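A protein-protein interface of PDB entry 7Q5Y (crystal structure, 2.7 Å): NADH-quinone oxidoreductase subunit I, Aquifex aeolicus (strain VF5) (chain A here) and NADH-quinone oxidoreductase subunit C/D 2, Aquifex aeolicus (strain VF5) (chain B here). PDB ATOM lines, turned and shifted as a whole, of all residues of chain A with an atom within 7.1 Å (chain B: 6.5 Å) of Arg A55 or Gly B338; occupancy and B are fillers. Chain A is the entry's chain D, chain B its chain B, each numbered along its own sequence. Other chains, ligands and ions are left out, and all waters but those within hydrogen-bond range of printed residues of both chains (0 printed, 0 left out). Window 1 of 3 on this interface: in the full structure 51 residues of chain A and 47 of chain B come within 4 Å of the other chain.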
ATOM      1  N   PRO A  50      12.801  12.953   8.211  1.00  0.00           N
ATOM      2  CA  PRO A  50      12.528  14.126   7.376  1.00  0.00           C
ATOM      3  C   PRO A  50      13.141  13.971   5.994  1.00  0.00           C
ATOM      4  O   PRO A  50      14.209  13.353   5.841  1.00  0.00           O
ATOM      5  CB  PRO A  50      13.196  15.277   8.153  1.00  0.00           C
ATOM      6  CG  PRO A  50      13.358  14.754   9.551  1.00  0.00           C
ATOM      7  CD  PRO A  50      13.594  13.291   9.405  1.00  0.00           C
ATOM      8  N   PRO A  51      12.505  14.516   4.958  1.00  0.00           N
ATOM      9  CA  PRO A  51      13.065  14.409   3.604  1.00  0.00           C
ATOM     10  C   PRO A  51      14.443  15.052   3.518  1.00  0.00           C
ATOM     11  O   PRO A  51      14.890  15.777   4.407  1.00  0.00           O
ATOM     12  CB  PRO A  51      12.049  15.157   2.729  1.00  0.00           C
ATOM     13  CG  PRO A  51      11.272  16.003   3.668  1.00  0.00           C
ATOM     14  CD  PRO A  51      11.224  15.238   4.963  1.00  0.00           C
ATOM     15  N   LYS A  52      15.127  14.770   2.408  1.00  0.00           N
ATOM     16  CA  LYS A  52      16.472  15.299   2.177  1.00  0.00           C
ATOM     17  C   LYS A  52      16.505  16.822   2.133  1.00  0.00           C
ATOM     18  O   LYS A  52      17.522  17.426   2.479  1.00  0.00           O
ATOM     19  CB  LYS A  52      17.021  14.732   0.867  1.00  0.00           C
ATOM     20  CG  LYS A  52      18.455  15.078   0.533  1.00  0.00           C
ATOM     21  CD  LYS A  52      19.452  14.150   1.205  1.00  0.00           C
ATOM     22  CE  LYS A  52      20.860  14.665   0.947  1.00  0.00           C
ATOM     23  NZ  LYS A  52      21.038  14.999  -0.502  1.00  0.00           N
ATOM     24  N   ARG A  53      15.422  17.460   1.695  1.00  0.00           N
ATOM     25  CA  ARG A  53      15.345  18.913   1.603  1.00  0.00           C
ATOM     26  C   ARG A  53      14.882  19.572   2.890  1.00  0.00           C
ATOM     27  O   ARG A  53      14.610  20.778   2.880  1.00  0.00           O
ATOM     28  CB  ARG A  53      14.400  19.339   0.476  1.00  0.00           C
ATOM     29  CG  ARG A  53      14.848  18.967  -0.916  1.00  0.00           C
ATOM     30  CD  ARG A  53      13.812  19.398  -1.923  1.00  0.00           C
ATOM     31  NE  ARG A  53      14.175  18.978  -3.269  1.00  0.00           N
ATOM     32  CZ  ARG A  53      13.571  19.401  -4.373  1.00  0.00           C
ATOM     33  NH1 ARG A  53      12.571  20.272  -4.303  1.00  0.00           N
ATOM     34  NH2 ARG A  53      13.977  18.957  -5.551  1.00  0.00           N
ATOM     35  N   PHE A  54      14.762  18.820   3.982  1.00  0.00           N
ATOM     36  CA  PHE A  54      14.288  19.399   5.233  1.00  0.00           C
ATOM     37  C   PHE A  54      15.191  20.537   5.701  1.00  0.00           C
ATOM     38  O   PHE A  54      16.424  20.453   5.646  1.00  0.00           O
ATOM     39  CB  PHE A  54      14.163  18.322   6.318  1.00  0.00           C
ATOM     40  CG  PHE A  54      13.477  18.805   7.575  1.00  0.00           C
ATOM     41  CD1 PHE A  54      12.166  19.258   7.527  1.00  0.00           C
ATOM     42  CD2 PHE A  54      14.124  18.781   8.800  1.00  0.00           C
ATOM     43  CE1 PHE A  54      11.524  19.713   8.665  1.00  0.00           C
ATOM     44  CE2 PHE A  54      13.481  19.220   9.944  1.00  0.00           C
ATOM     45  CZ  PHE A  54      12.178  19.686   9.875  1.00  0.00           C
ATOM     46  N   ARG A  55      14.546  21.611   6.160  1.00  0.00           N
ATOM     47  CA  ARG A  55      15.206  22.811   6.664  1.00  0.00           C
ATOM     48  C   ARG A  55      15.234  22.722   8.188  1.00  0.00           C
ATOM     49  O   ARG A  55      14.440  23.348   8.890  1.00  0.00           O
ATOM     50  CB  ARG A  55      14.469  24.061   6.189  1.00  0.00           C
ATOM     51  CG  ARG A  55      14.898  24.603   4.827  1.00  0.00           C
ATOM     52  CD  ARG A  55      13.758  25.266   4.075  1.00  0.00           C
ATOM     53  NE  ARG A  55      12.941  26.164   4.885  1.00  0.00           N
ATOM     54  CZ  ARG A  55      11.696  26.512   4.556  1.00  0.00           C
ATOM     55  NH1 ARG A  55      11.162  26.015   3.451  1.00  0.00           N
ATOM     56  NH2 ARG A  55      10.974  27.329   5.326  1.00  0.00           N
ATOM     57  N   GLY A  56      16.157  21.910   8.703  1.00  0.00           N
ATOM     58  CA  GLY A  56      16.329  21.717  10.133  1.00  0.00           C
ATOM     59  C   GLY A  56      17.392  22.616  10.739  1.00  0.00           C
ATOM     60  O   GLY A  56      17.659  23.721  10.257  1.00  0.00           O
ATOM     61  N   ALA A  57      18.007  22.135  11.815  1.00  0.00           N
ATOM     62  CA  ALA A  57      19.041  22.909  12.485  1.00  0.00           C
ATOM     63  C   ALA A  57      20.184  23.200  11.526  1.00  0.00           C
ATOM     64  O   ALA A  57      20.617  22.328  10.769  1.00  0.00           O
ATOM     65  CB  ALA A  57      19.565  22.159  13.710  1.00  0.00           C
ATOM     66  N   HIS A  58      20.679  24.435  11.569  1.00  0.00           N
ATOM     67  CA  HIS A  58      21.756  24.835  10.683  1.00  0.00           C
ATOM     68  C   HIS A  58      23.034  24.067  10.997  1.00  0.00           C
ATOM     69  O   HIS A  58      23.195  23.479  12.066  1.00  0.00           O
ATOM     70  CB  HIS A  58      22.027  26.327  10.788  1.00  0.00           C
ATOM     71  CG  HIS A  58      20.815  27.177  10.619  1.00  0.00           C
ATOM     72  ND1 HIS A  58      20.641  28.019   9.539  1.00  0.00           N
ATOM     73  CD2 HIS A  58      19.728  27.344  11.409  1.00  0.00           C
ATOM     74  CE1 HIS A  58      19.493  28.662   9.668  1.00  0.00           C
ATOM     75  NE2 HIS A  58      18.920  28.269  10.793  1.00  0.00           N
ATOM     76  N   LEU A 128      13.380  31.993  11.314  1.00  0.00           N
ATOM     77  CA  LEU A 128      12.209  31.657  10.515  1.00  0.00           C
ATOM     78  C   LEU A 128      12.335  30.286   9.868  1.00  0.00           C
ATOM     79  O   LEU A 128      11.336  29.774   9.358  1.00  0.00           O
ATOM     80  CB  LEU A 128      12.011  32.697   9.403  1.00  0.00           C
ATOM     81  CG  LEU A 128      11.625  34.145   9.701  1.00  0.00           C
ATOM     82  CD1 LEU A 128      12.358  35.076   8.744  1.00  0.00           C
ATOM     83  CD2 LEU A 128      10.140  34.339   9.521  1.00  0.00           C
ATOM     84  N   PHE A 129      13.543  29.695   9.877  1.00  0.00           N
ATOM     85  CA  PHE A 129      13.821  28.407   9.235  1.00  0.00           C
ATOM     86  C   PHE A 129      13.381  28.500   7.781  1.00  0.00           C
ATOM     87  O   PHE A 129      12.818  27.575   7.195  1.00  0.00           O
ATOM     88  CB  PHE A 129      13.162  27.252   9.994  1.00  0.00           C
ATOM     89  CG  PHE A 129      13.852  26.936  11.280  1.00  0.00           C
ATOM     90  CD1 PHE A 129      13.582  27.678  12.425  1.00  0.00           C
ATOM     91  CD2 PHE A 129      14.785  25.917  11.348  1.00  0.00           C
ATOM     92  CE1 PHE A 129      14.246  27.425  13.608  1.00  0.00           C
ATOM     93  CE2 PHE A 129      15.448  25.649  12.530  1.00  0.00           C
ATOM     94  CZ  PHE A 129      15.183  26.411  13.657  1.00  0.00           C
ATOM     95  N   CYS A 130      13.676  29.660   7.208  1.00  0.00           N
ATOM     96  CA  CYS A 130      13.291  30.049   5.865  1.00  0.00           C
ATOM     97  C   CYS A 130      14.266  29.588   4.780  1.00  0.00           C
ATOM     98  O   CYS A 130      13.836  29.355   3.643  1.00  0.00           O
ATOM     99  CB  CYS A 130      13.107  31.570   5.878  1.00  0.00           C
ATOM    100  SG  CYS A 130      14.624  32.498   5.729  1.00  0.00           S
ATOM    101  N   GLY A 131      15.552  29.423   5.100  1.00  0.00           N
ATOM    102  CA  GLY A 131      16.558  28.966   4.162  1.00  0.00           C
ATOM    103  C   GLY A 131      17.233  30.035   3.325  1.00  0.00           C
ATOM    104  O   GLY A 131      18.081  29.695   2.488  1.00  0.00           O
ATOM    105  N   LEU A 132      16.888  31.311   3.523  1.00  0.00           N
ATOM    106  CA  LEU A 132      17.474  32.388   2.735  1.00  0.00           C
ATOM    107  C   LEU A 132      18.980  32.491   2.909  1.00  0.00           C
ATOM    108  O   LEU A 132      19.691  32.867   1.962  1.00  0.00           O
ATOM    109  CB  LEU A 132      16.829  33.719   3.120  1.00  0.00           C
ATOM    110  CG  LEU A 132      15.348  33.880   2.771  1.00  0.00           C
ATOM    111  CD1 LEU A 132      14.873  35.325   2.994  1.00  0.00           C
ATOM    112  CD2 LEU A 132      15.000  33.348   1.365  1.00  0.00           C
ATOM    113  N   VAL A 134      21.165  29.967   3.530  1.00  0.00           N
ATOM    114  CA  VAL A 134      21.847  28.916   2.784  1.00  0.00           C
ATOM    115  C   VAL A 134      21.942  29.309   1.318  1.00  0.00           C
ATOM    116  O   VAL A 134      22.962  29.058   0.646  1.00  0.00           O
ATOM    117  CB  VAL A 134      21.131  27.568   2.962  1.00  0.00           C
ATOM    118  CG1 VAL A 134      21.816  26.522   2.108  1.00  0.00           C
ATOM    119  CG2 VAL A 134      21.125  27.143   4.430  1.00  0.00           C
ATOM    120  N   MET A 144      21.245  23.443   6.180  1.00  0.00           N
ATOM    121  CA  MET A 144      20.183  23.042   7.097  1.00  0.00           C
ATOM    122  C   MET A 144      20.198  21.517   7.139  1.00  0.00           C
ATOM    123  O   MET A 144      20.093  20.862   6.091  1.00  0.00           O
ATOM    124  CB  MET A 144      18.800  23.526   6.651  1.00  0.00           C
ATOM    125  CG  MET A 144      18.669  24.975   6.175  1.00  0.00           C
ATOM    126  SD  MET A 144      18.283  26.168   7.458  1.00  0.00           S
ATOM    127  CE  MET A 144      16.536  26.498   7.305  1.00  0.00           C
ATOM    128  N   THR A 145      20.328  20.961   8.340  1.00  0.00           N
ATOM    129  CA  THR A 145      20.365  19.522   8.540  1.00  0.00           C
ATOM    130  C   THR A 145      18.950  19.002   8.798  1.00  0.00           C
ATOM    131  O   THR A 145      17.953  19.718   8.662  1.00  0.00           O
ATOM    132  CB  THR A 145      21.278  19.164   9.715  1.00  0.00           C
ATOM    133  OG1 THR A 145      20.744  19.721  10.927  1.00  0.00           O
ATOM    134  CG2 THR A 145      22.694  19.701   9.509  1.00  0.00           C
ATOM    135  N   ASP A 146      18.856  17.740   9.205  1.00  0.00           N
ATOM    136  CA  ASP A 146      17.591  17.112   9.529  1.00  0.00           C
ATOM    137  C   ASP A 146      17.352  17.118  11.026  1.00  0.00           C
ATOM    138  O   ASP A 146      16.355  16.564  11.492  1.00  0.00           O
ATOM    139  CB  ASP A 146      17.550  15.669   9.007  1.00  0.00           C
ATOM    140  CG  ASP A 146      18.679  14.800   9.552  1.00  0.00           C
ATOM    141  OD1 ASP A 146      19.525  15.279  10.334  1.00  0.00           O
ATOM    142  OD2 ASP A 146      18.701  13.600   9.214  1.00  0.00           O
ATOM    143  N   ILE A 147      18.264  17.722  11.780  1.00  0.00           N
ATOM    144  CA  ILE A 147      18.175  17.776  13.229  1.00  0.00           C
ATOM    145  C   ILE A 147      16.999  18.651  13.640  1.00  0.00           C
ATOM    146  O   ILE A 147      16.921  19.825  13.267  1.00  0.00           O
ATOM    147  CB  ILE A 147      19.498  18.280  13.812  1.00  0.00           C
ATOM    148  CG1 ILE A 147      20.603  17.272  13.483  1.00  0.00           C
ATOM    149  CG2 ILE A 147      19.395  18.516  15.315  1.00  0.00           C
ATOM    150  CD1 ILE A 147      21.990  17.804  13.711  1.00  0.00           C
ATOM    151  N   ASP B 256       4.184  33.784   4.295  1.00  0.00           N
ATOM    152  CA  ASP B 256       3.713  32.476   4.747  1.00  0.00           C
ATOM    153  C   ASP B 256       3.015  32.587   6.077  1.00  0.00           C
ATOM    154  O   ASP B 256       2.090  31.828   6.360  1.00  0.00           O
ATOM    155  CB  ASP B 256       4.852  31.477   4.962  1.00  0.00           C
ATOM    156  CG  ASP B 256       5.600  31.151   3.716  1.00  0.00           C
ATOM    157  OD1 ASP B 256       5.447  31.887   2.728  1.00  0.00           O
ATOM    158  OD2 ASP B 256       6.323  30.134   3.725  1.00  0.00           O
ATOM    159  N   ARG B 257       3.456  33.519   6.908  1.00  0.00           N
ATOM    160  CA  ARG B 257       2.927  33.687   8.245  1.00  0.00           C
ATOM    161  C   ARG B 257       1.757  34.661   8.310  1.00  0.00           C
ATOM    162  O   ARG B 257       1.477  35.203   9.386  1.00  0.00           O
ATOM    163  CB  ARG B 257       4.070  34.077   9.181  1.00  0.00           C
ATOM    164  CG  ARG B 257       5.042  32.894   9.327  1.00  0.00           C
ATOM    165  CD  ARG B 257       6.514  33.283   9.434  1.00  0.00           C
ATOM    166  NE  ARG B 257       7.380  32.101   9.568  1.00  0.00           N
ATOM    167  CZ  ARG B 257       7.965  31.456   8.555  1.00  0.00           C
ATOM    168  NH1 ARG B 257       7.806  31.862   7.296  1.00  0.00           N
ATOM    169  NH2 ARG B 257       8.724  30.396   8.801  1.00  0.00           N
ATOM    170  N   ILE B 333       4.486  18.667   0.024  1.00  0.00           N
ATOM    171  CA  ILE B 333       5.027  20.017   0.169  1.00  0.00           C
ATOM    172  C   ILE B 333       6.336  19.996   0.959  1.00  0.00           C
ATOM    173  O   ILE B 333       7.330  20.610   0.560  1.00  0.00           O
ATOM    174  CB  ILE B 333       3.971  20.935   0.816  1.00  0.00           C
ATOM    175  CG1 ILE B 333       2.805  21.143  -0.139  1.00  0.00           C
ATOM    176  CG2 ILE B 333       4.549  22.264   1.220  1.00  0.00           C
ATOM    177  CD1 ILE B 333       1.667  21.879   0.484  1.00  0.00           C
ATOM    178  N   GLU B 334       6.363  19.279   2.083  1.00  0.00           N
ATOM    179  CA  GLU B 334       7.583  19.212   2.881  1.00  0.00           C
ATOM    180  C   GLU B 334       8.732  18.592   2.103  1.00  0.00           C
ATOM    181  O   GLU B 334       9.875  19.050   2.197  1.00  0.00           O
ATOM    182  CB  GLU B 334       7.340  18.412   4.161  1.00  0.00           C
ATOM    183  CG  GLU B 334       8.566  18.322   5.058  1.00  0.00           C
ATOM    184  CD  GLU B 334       8.388  17.348   6.204  1.00  0.00           C
ATOM    185  OE1 GLU B 334       7.578  16.380   6.078  1.00  0.00           O
ATOM    186  OE2 GLU B 334       9.079  17.557   7.229  1.00  0.00           O
ATOM    187  N   GLY B 335       8.454  17.553   1.320  1.00  0.00           N
ATOM    188  CA  GLY B 335       9.525  16.925   0.573  1.00  0.00           C
ATOM    189  C   GLY B 335      10.129  17.817  -0.493  1.00  0.00           C
ATOM    190  O   GLY B 335      11.323  17.699  -0.793  1.00  0.00           O
ATOM    191  N   ASN B 336       9.329  18.734  -1.057  1.00  0.00           N
ATOM    192  CA  ASN B 336       9.756  19.641  -2.122  1.00  0.00           C
ATOM    193  C   ASN B 336      10.209  21.014  -1.631  1.00  0.00           C
ATOM    194  O   ASN B 336      11.252  21.503  -2.069  1.00  0.00           O
ATOM    195  CB  ASN B 336       8.621  19.822  -3.140  1.00  0.00           C
ATOM    196  CG  ASN B 336       8.502  18.654  -4.101  1.00  0.00           C
ATOM    197  OD1 ASN B 336       9.185  18.616  -5.133  1.00  0.00           O
ATOM    198  ND2 ASN B 336       7.628  17.689  -3.769  1.00  0.00           N
ATOM    199  N   ALA B 337       9.451  21.647  -0.730  1.00  0.00           N
ATOM    200  CA  ALA B 337       9.828  22.966  -0.228  1.00  0.00           C
ATOM    201  C   ALA B 337      10.833  22.871   0.916  1.00  0.00           C
ATOM    202  O   ALA B 337      11.719  23.726   1.043  1.00  0.00           O
ATOM    203  CB  ALA B 337       8.585  23.745   0.211  1.00  0.00           C
ATOM    204  N   GLY B 338      10.705  21.855   1.764  1.00  0.00           N
ATOM    205  CA  GLY B 338      11.596  21.651   2.888  1.00  0.00           C
ATOM    206  C   GLY B 338      10.980  21.926   4.244  1.00  0.00           C
ATOM    207  O   GLY B 338      11.631  21.659   5.262  1.00  0.00           O
ATOM    208  N   TYR B 339       9.753  22.449   4.293  1.00  0.00           N
ATOM    209  CA  TYR B 339       9.066  22.745   5.541  1.00  0.00           C
ATOM    210  C   TYR B 339       7.597  22.365   5.376  1.00  0.00           C
ATOM    211  O   TYR B 339       7.035  22.465   4.284  1.00  0.00           O
ATOM    212  CB  TYR B 339       9.270  24.224   5.950  1.00  0.00           C
ATOM    213  CG  TYR B 339       9.739  24.356   7.390  1.00  0.00           C
ATOM    214  CD1 TYR B 339      10.855  23.665   7.833  1.00  0.00           C
ATOM    215  CD2 TYR B 339       9.051  25.140   8.308  1.00  0.00           C
ATOM    216  CE1 TYR B 339      11.280  23.751   9.142  1.00  0.00           C
ATOM    217  CE2 TYR B 339       9.472  25.235   9.623  1.00  0.00           C
ATOM    218  CZ  TYR B 339      10.588  24.536  10.038  1.00  0.00           C
ATOM    219  OH  TYR B 339      11.021  24.617  11.348  1.00  0.00           O
ATOM    220  N   ARG B 340       6.984  21.903   6.471  1.00  0.00           N
ATOM    221  CA  ARG B 340       5.599  21.426   6.407  1.00  0.00           C
ATOM    222  C   ARG B 340       4.587  22.553   6.221  1.00  0.00           C
ATOM    223  O   ARG B 340       3.744  22.491   5.320  1.00  0.00           O
ATOM    224  CB  ARG B 340       5.262  20.592   7.650  1.00  0.00           C
ATOM    225  CG  ARG B 340       6.003  19.271   7.724  1.00  0.00           C
ATOM    226  CD  ARG B 340       5.623  18.428   8.942  1.00  0.00           C
ATOM    227  NE  ARG B 340       4.570  17.450   8.700  1.00  0.00           N
ATOM    228  CZ  ARG B 340       3.362  17.501   9.247  1.00  0.00           C
ATOM    229  NH1 ARG B 340       3.038  18.473  10.079  1.00  0.00           N
ATOM    230  NH2 ARG B 340       2.477  16.567   8.973  1.00  0.00           N
ATOM    231  N   THR B 342       5.179  26.472   6.779  1.00  0.00           N
ATOM    232  CA  THR B 342       5.738  27.678   6.159  1.00  0.00           C
ATOM    233  C   THR B 342       6.727  27.250   5.077  1.00  0.00           C
ATOM    234  O   THR B 342       7.949  27.316   5.233  1.00  0.00           O
ATOM    235  CB  THR B 342       6.367  28.554   7.219  1.00  0.00           C
ATOM    236  OG1 THR B 342       7.039  27.704   8.150  1.00  0.00           O
ATOM    237  CG2 THR B 342       5.291  29.346   7.939  1.00  0.00           C
ATOM    238  N   SER B 343       6.150  26.814   3.952  1.00  0.00           N
ATOM    239  CA  SER B 343       6.881  26.281   2.802  1.00  0.00           C
ATOM    240  C   SER B 343       8.076  27.124   2.372  1.00  0.00           C
ATOM    241  O   SER B 343       9.194  26.610   2.267  1.00  0.00           O
ATOM    242  CB  SER B 343       5.927  26.109   1.617  1.00  0.00           C
ATOM    243  OG  SER B 343       4.799  25.352   1.991  1.00  0.00           O
ATOM    244  N   CYS B 344       7.850  28.406   2.064  1.00  0.00           N
ATOM    245  CA  CYS B 344       8.908  29.277   1.549  1.00  0.00           C
ATOM    246  C   CYS B 344       9.480  28.610   0.297  1.00  0.00           C
ATOM    247  O   CYS B 344      10.678  28.344   0.175  1.00  0.00           O
ATOM    248  CB  CYS B 344       9.986  29.571   2.595  1.00  0.00           C
ATOM    249  SG  CYS B 344      11.078  30.940   2.177  1.00  0.00           S
ATOM    250  N   PHE B 345       8.571  28.287  -0.622  1.00  0.00           N
ATOM    251  CA  PHE B 345       8.862  27.602  -1.870  1.00  0.00           C
ATOM    252  C   PHE B 345       9.044  28.559  -3.033  1.00  0.00           C
ATOM    253  O   PHE B 345       9.946  28.369  -3.857  1.00  0.00           O
ATOM    254  CB  PHE B 345       7.735  26.613  -2.178  1.00  0.00           C
ATOM    255  CG  PHE B 345       8.048  25.655  -3.282  1.00  0.00           C
ATOM    256  CD1 PHE B 345       9.335  25.139  -3.431  1.00  0.00           C
ATOM    257  CD2 PHE B 345       7.040  25.191  -4.114  1.00  0.00           C
ATOM    258  CE1 PHE B 345       9.626  24.224  -4.439  1.00  0.00           C
ATOM    259  CE2 PHE B 345       7.317  24.263  -5.111  1.00  0.00           C
ATOM    260  CZ  PHE B 345       8.612  23.780  -5.277  1.00  0.00           C
ATOM    261  N   ARG B 347      10.051  31.957  -5.116  1.00  0.00           N
ATOM    262  CA  ARG B 347      11.133  32.922  -5.155  1.00  0.00           C
ATOM    263  C   ARG B 347      10.766  33.922  -6.232  1.00  0.00           C
ATOM    264  O   ARG B 347      10.003  33.614  -7.149  1.00  0.00           O
ATOM    265  CB  ARG B 347      12.486  32.287  -5.491  1.00  0.00           C
ATOM    266  CG  ARG B 347      13.136  31.425  -4.410  1.00  0.00           C
ATOM    267  CD  ARG B 347      13.411  32.173  -3.113  1.00  0.00           C
ATOM    268  NE  ARG B 347      12.842  31.481  -1.950  1.00  0.00           N
ATOM    269  CZ  ARG B 347      13.527  30.655  -1.163  1.00  0.00           C
ATOM    270  NH1 ARG B 347      14.811  30.423  -1.398  1.00  0.00           N
ATOM    271  NH2 ARG B 347      12.945  30.077  -0.123  1.00  0.00           N
ATOM    272  N   HIS B 352      11.869  27.853  -5.720  1.00  0.00           N
ATOM    273  CA  HIS B 352      13.147  27.621  -5.049  1.00  0.00           C
ATOM    274  C   HIS B 352      13.928  26.484  -5.698  1.00  0.00           C
ATOM    275  O   HIS B 352      15.087  26.657  -6.090  1.00  0.00           O
ATOM    276  CB  HIS B 352      12.895  27.333  -3.570  1.00  0.00           C
ATOM    277  CG  HIS B 352      14.130  27.330  -2.729  1.00  0.00           C
ATOM    278  ND1 HIS B 352      15.377  27.619  -3.238  1.00  0.00           N
ATOM    279  CD2 HIS B 352      14.312  27.056  -1.415  1.00  0.00           C
ATOM    280  CE1 HIS B 352      16.273  27.533  -2.273  1.00  0.00           C
ATOM    281  NE2 HIS B 352      15.653  27.193  -1.156  1.00  0.00           N
ATOM    282  N   TYR B 353      13.317  25.307  -5.798  1.00  0.00           N
ATOM    283  CA  TYR B 353      13.942  24.147  -6.411  1.00  0.00           C
ATOM    284  C   TYR B 353      13.002  23.514  -7.420  1.00  0.00           C
ATOM    285  O   TYR B 353      11.814  23.836  -7.502  1.00  0.00           O
ATOM    286  CB  TYR B 353      14.304  23.027  -5.419  1.00  0.00           C
ATOM    287  CG  TYR B 353      14.759  23.378  -4.032  1.00  0.00           C
ATOM    288  CD1 TYR B 353      16.106  23.660  -3.772  1.00  0.00           C
ATOM    289  CD2 TYR B 353      13.873  23.353  -2.966  1.00  0.00           C
ATOM    290  CE1 TYR B 353      16.548  23.946  -2.499  1.00  0.00           C
ATOM    291  CE2 TYR B 353      14.302  23.643  -1.685  1.00  0.00           C
ATOM    292  CZ  TYR B 353      15.643  23.938  -1.457  1.00  0.00           C
ATOM    293  OH  TYR B 353      16.077  24.221  -0.181  1.00  0.00           O
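The guanidinium group (NH2) of Arg B257 lies within hydrogen-bond range of the backbone carbonyl oxygen (O) of Leu A128.
The guanidinium group (NH1) of Arg A53 sits at hydrogen-bond distance from the backbone carbonyl oxygen (O) of Asn B336 (2.9 Å).
The backbone carbonyl oxygen (O) of Ala B337 sits at hydrogen-bond distance from the guanidinium group (NH1) of Arg A55, at 3.4 Å.
The backbone NH of Arg A55 lies within hydrogen-bond range of the backbone carbonyl oxygen of Gly B338 (3.1 Å).
The backbone carbonyl oxygen (O) of Thr B342 sits at hydrogen-bond distance from the guanidinium group (NH2) of Arg A55 (3.0 Å).
The side-chain sulfur (SG) of Cys B344 is in hydrogen-bond range of the backbone carbonyl oxygen (O) of Cys A130.
The backbone carbonyl oxygen (O) of Ser B343 sits close to the guanidinium group (NH1) of Arg A55 (2.4 Å).
The side-chain carboxylate of Asp B256 is in hydrogen-bond range of the backbone NH of Cys B344, 2.8 Å away.
The guanidinium group (NH2) of Arg B257 lies within hydrogen-bond range of the side-chain hydroxyl (OG1) of Thr B342 (3.2 Å).
The guanidinium group (NH2) of Arg B347 lies within hydrogen-bond range of the backbone carbonyl oxygen (O) of Cys B344, at 2.9 Å.
A ring nitrogen (NE2) of His B352 sits at hydrogen-bond distance from the guanidinium group (NH1) of Arg B347 (3.3 Å).
A ring nitrogen (NE2) of His B352 lies within hydrogen-bond range of the side-chain hydroxyl (OH) of Tyr B353, 3.2 Å away.
The backbone NH (N) of Leu A132 lies close to the side-chain sulfur (SG) of Cys A130 (3.4 Å).
CG of Pro A51 touches CA of Gly B335, at 3.7 Å.
CD of Arg A53 touches O of Gly B335, at 3.2 Å.
Gly B338 touches Arg A53 (CA to O, 3.1 Å).
NH1 of Arg A53 touches CB of Tyr B353, 3.4 Å away.
CD1 of Phe A54 touches OE2 of Glu B334, 3.5 Å away.
Arg A55 touches Tyr B339.
Cys B344 touches Arg A55 (CB to NH2, 3.7 Å).
OH of Tyr B339 touches CB of Phe A129, at 3.7 Å.
Cys A130 touches Arg B347.
Arg B347 touches Leu A132.
Arg A55 touches just these residues of chain B: Ala B337, Gly B338, Tyr B339, Thr B342, Ser B343 and Cys B344.
Gly B338 touches just these residues of chain A: Arg A53, Phe A54 and Arg A55.
Of the printed residues of chain A, Arg B257 touches Leu A128 (2.7 Å).
Of the printed residues of chain B, Phe A129 touches Tyr B339.
Gly A56 touches none of the printed residues of chain B.
Of the 17 printed residues of chain B, 12 touch a printed residue of chain A.
Hydrophobic or aromatic side chains of chain A that line the printed part of chain B: Pro A51, Phe A54, Leu A128, Phe A129 and Leu A132.
Among the printed residues, 19 pairs touch across the chains.
Among the printed residues, no Asp or Glu carboxylate lies within 4 Å of a Lys or Arg side-chain nitrogen of the other chain.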
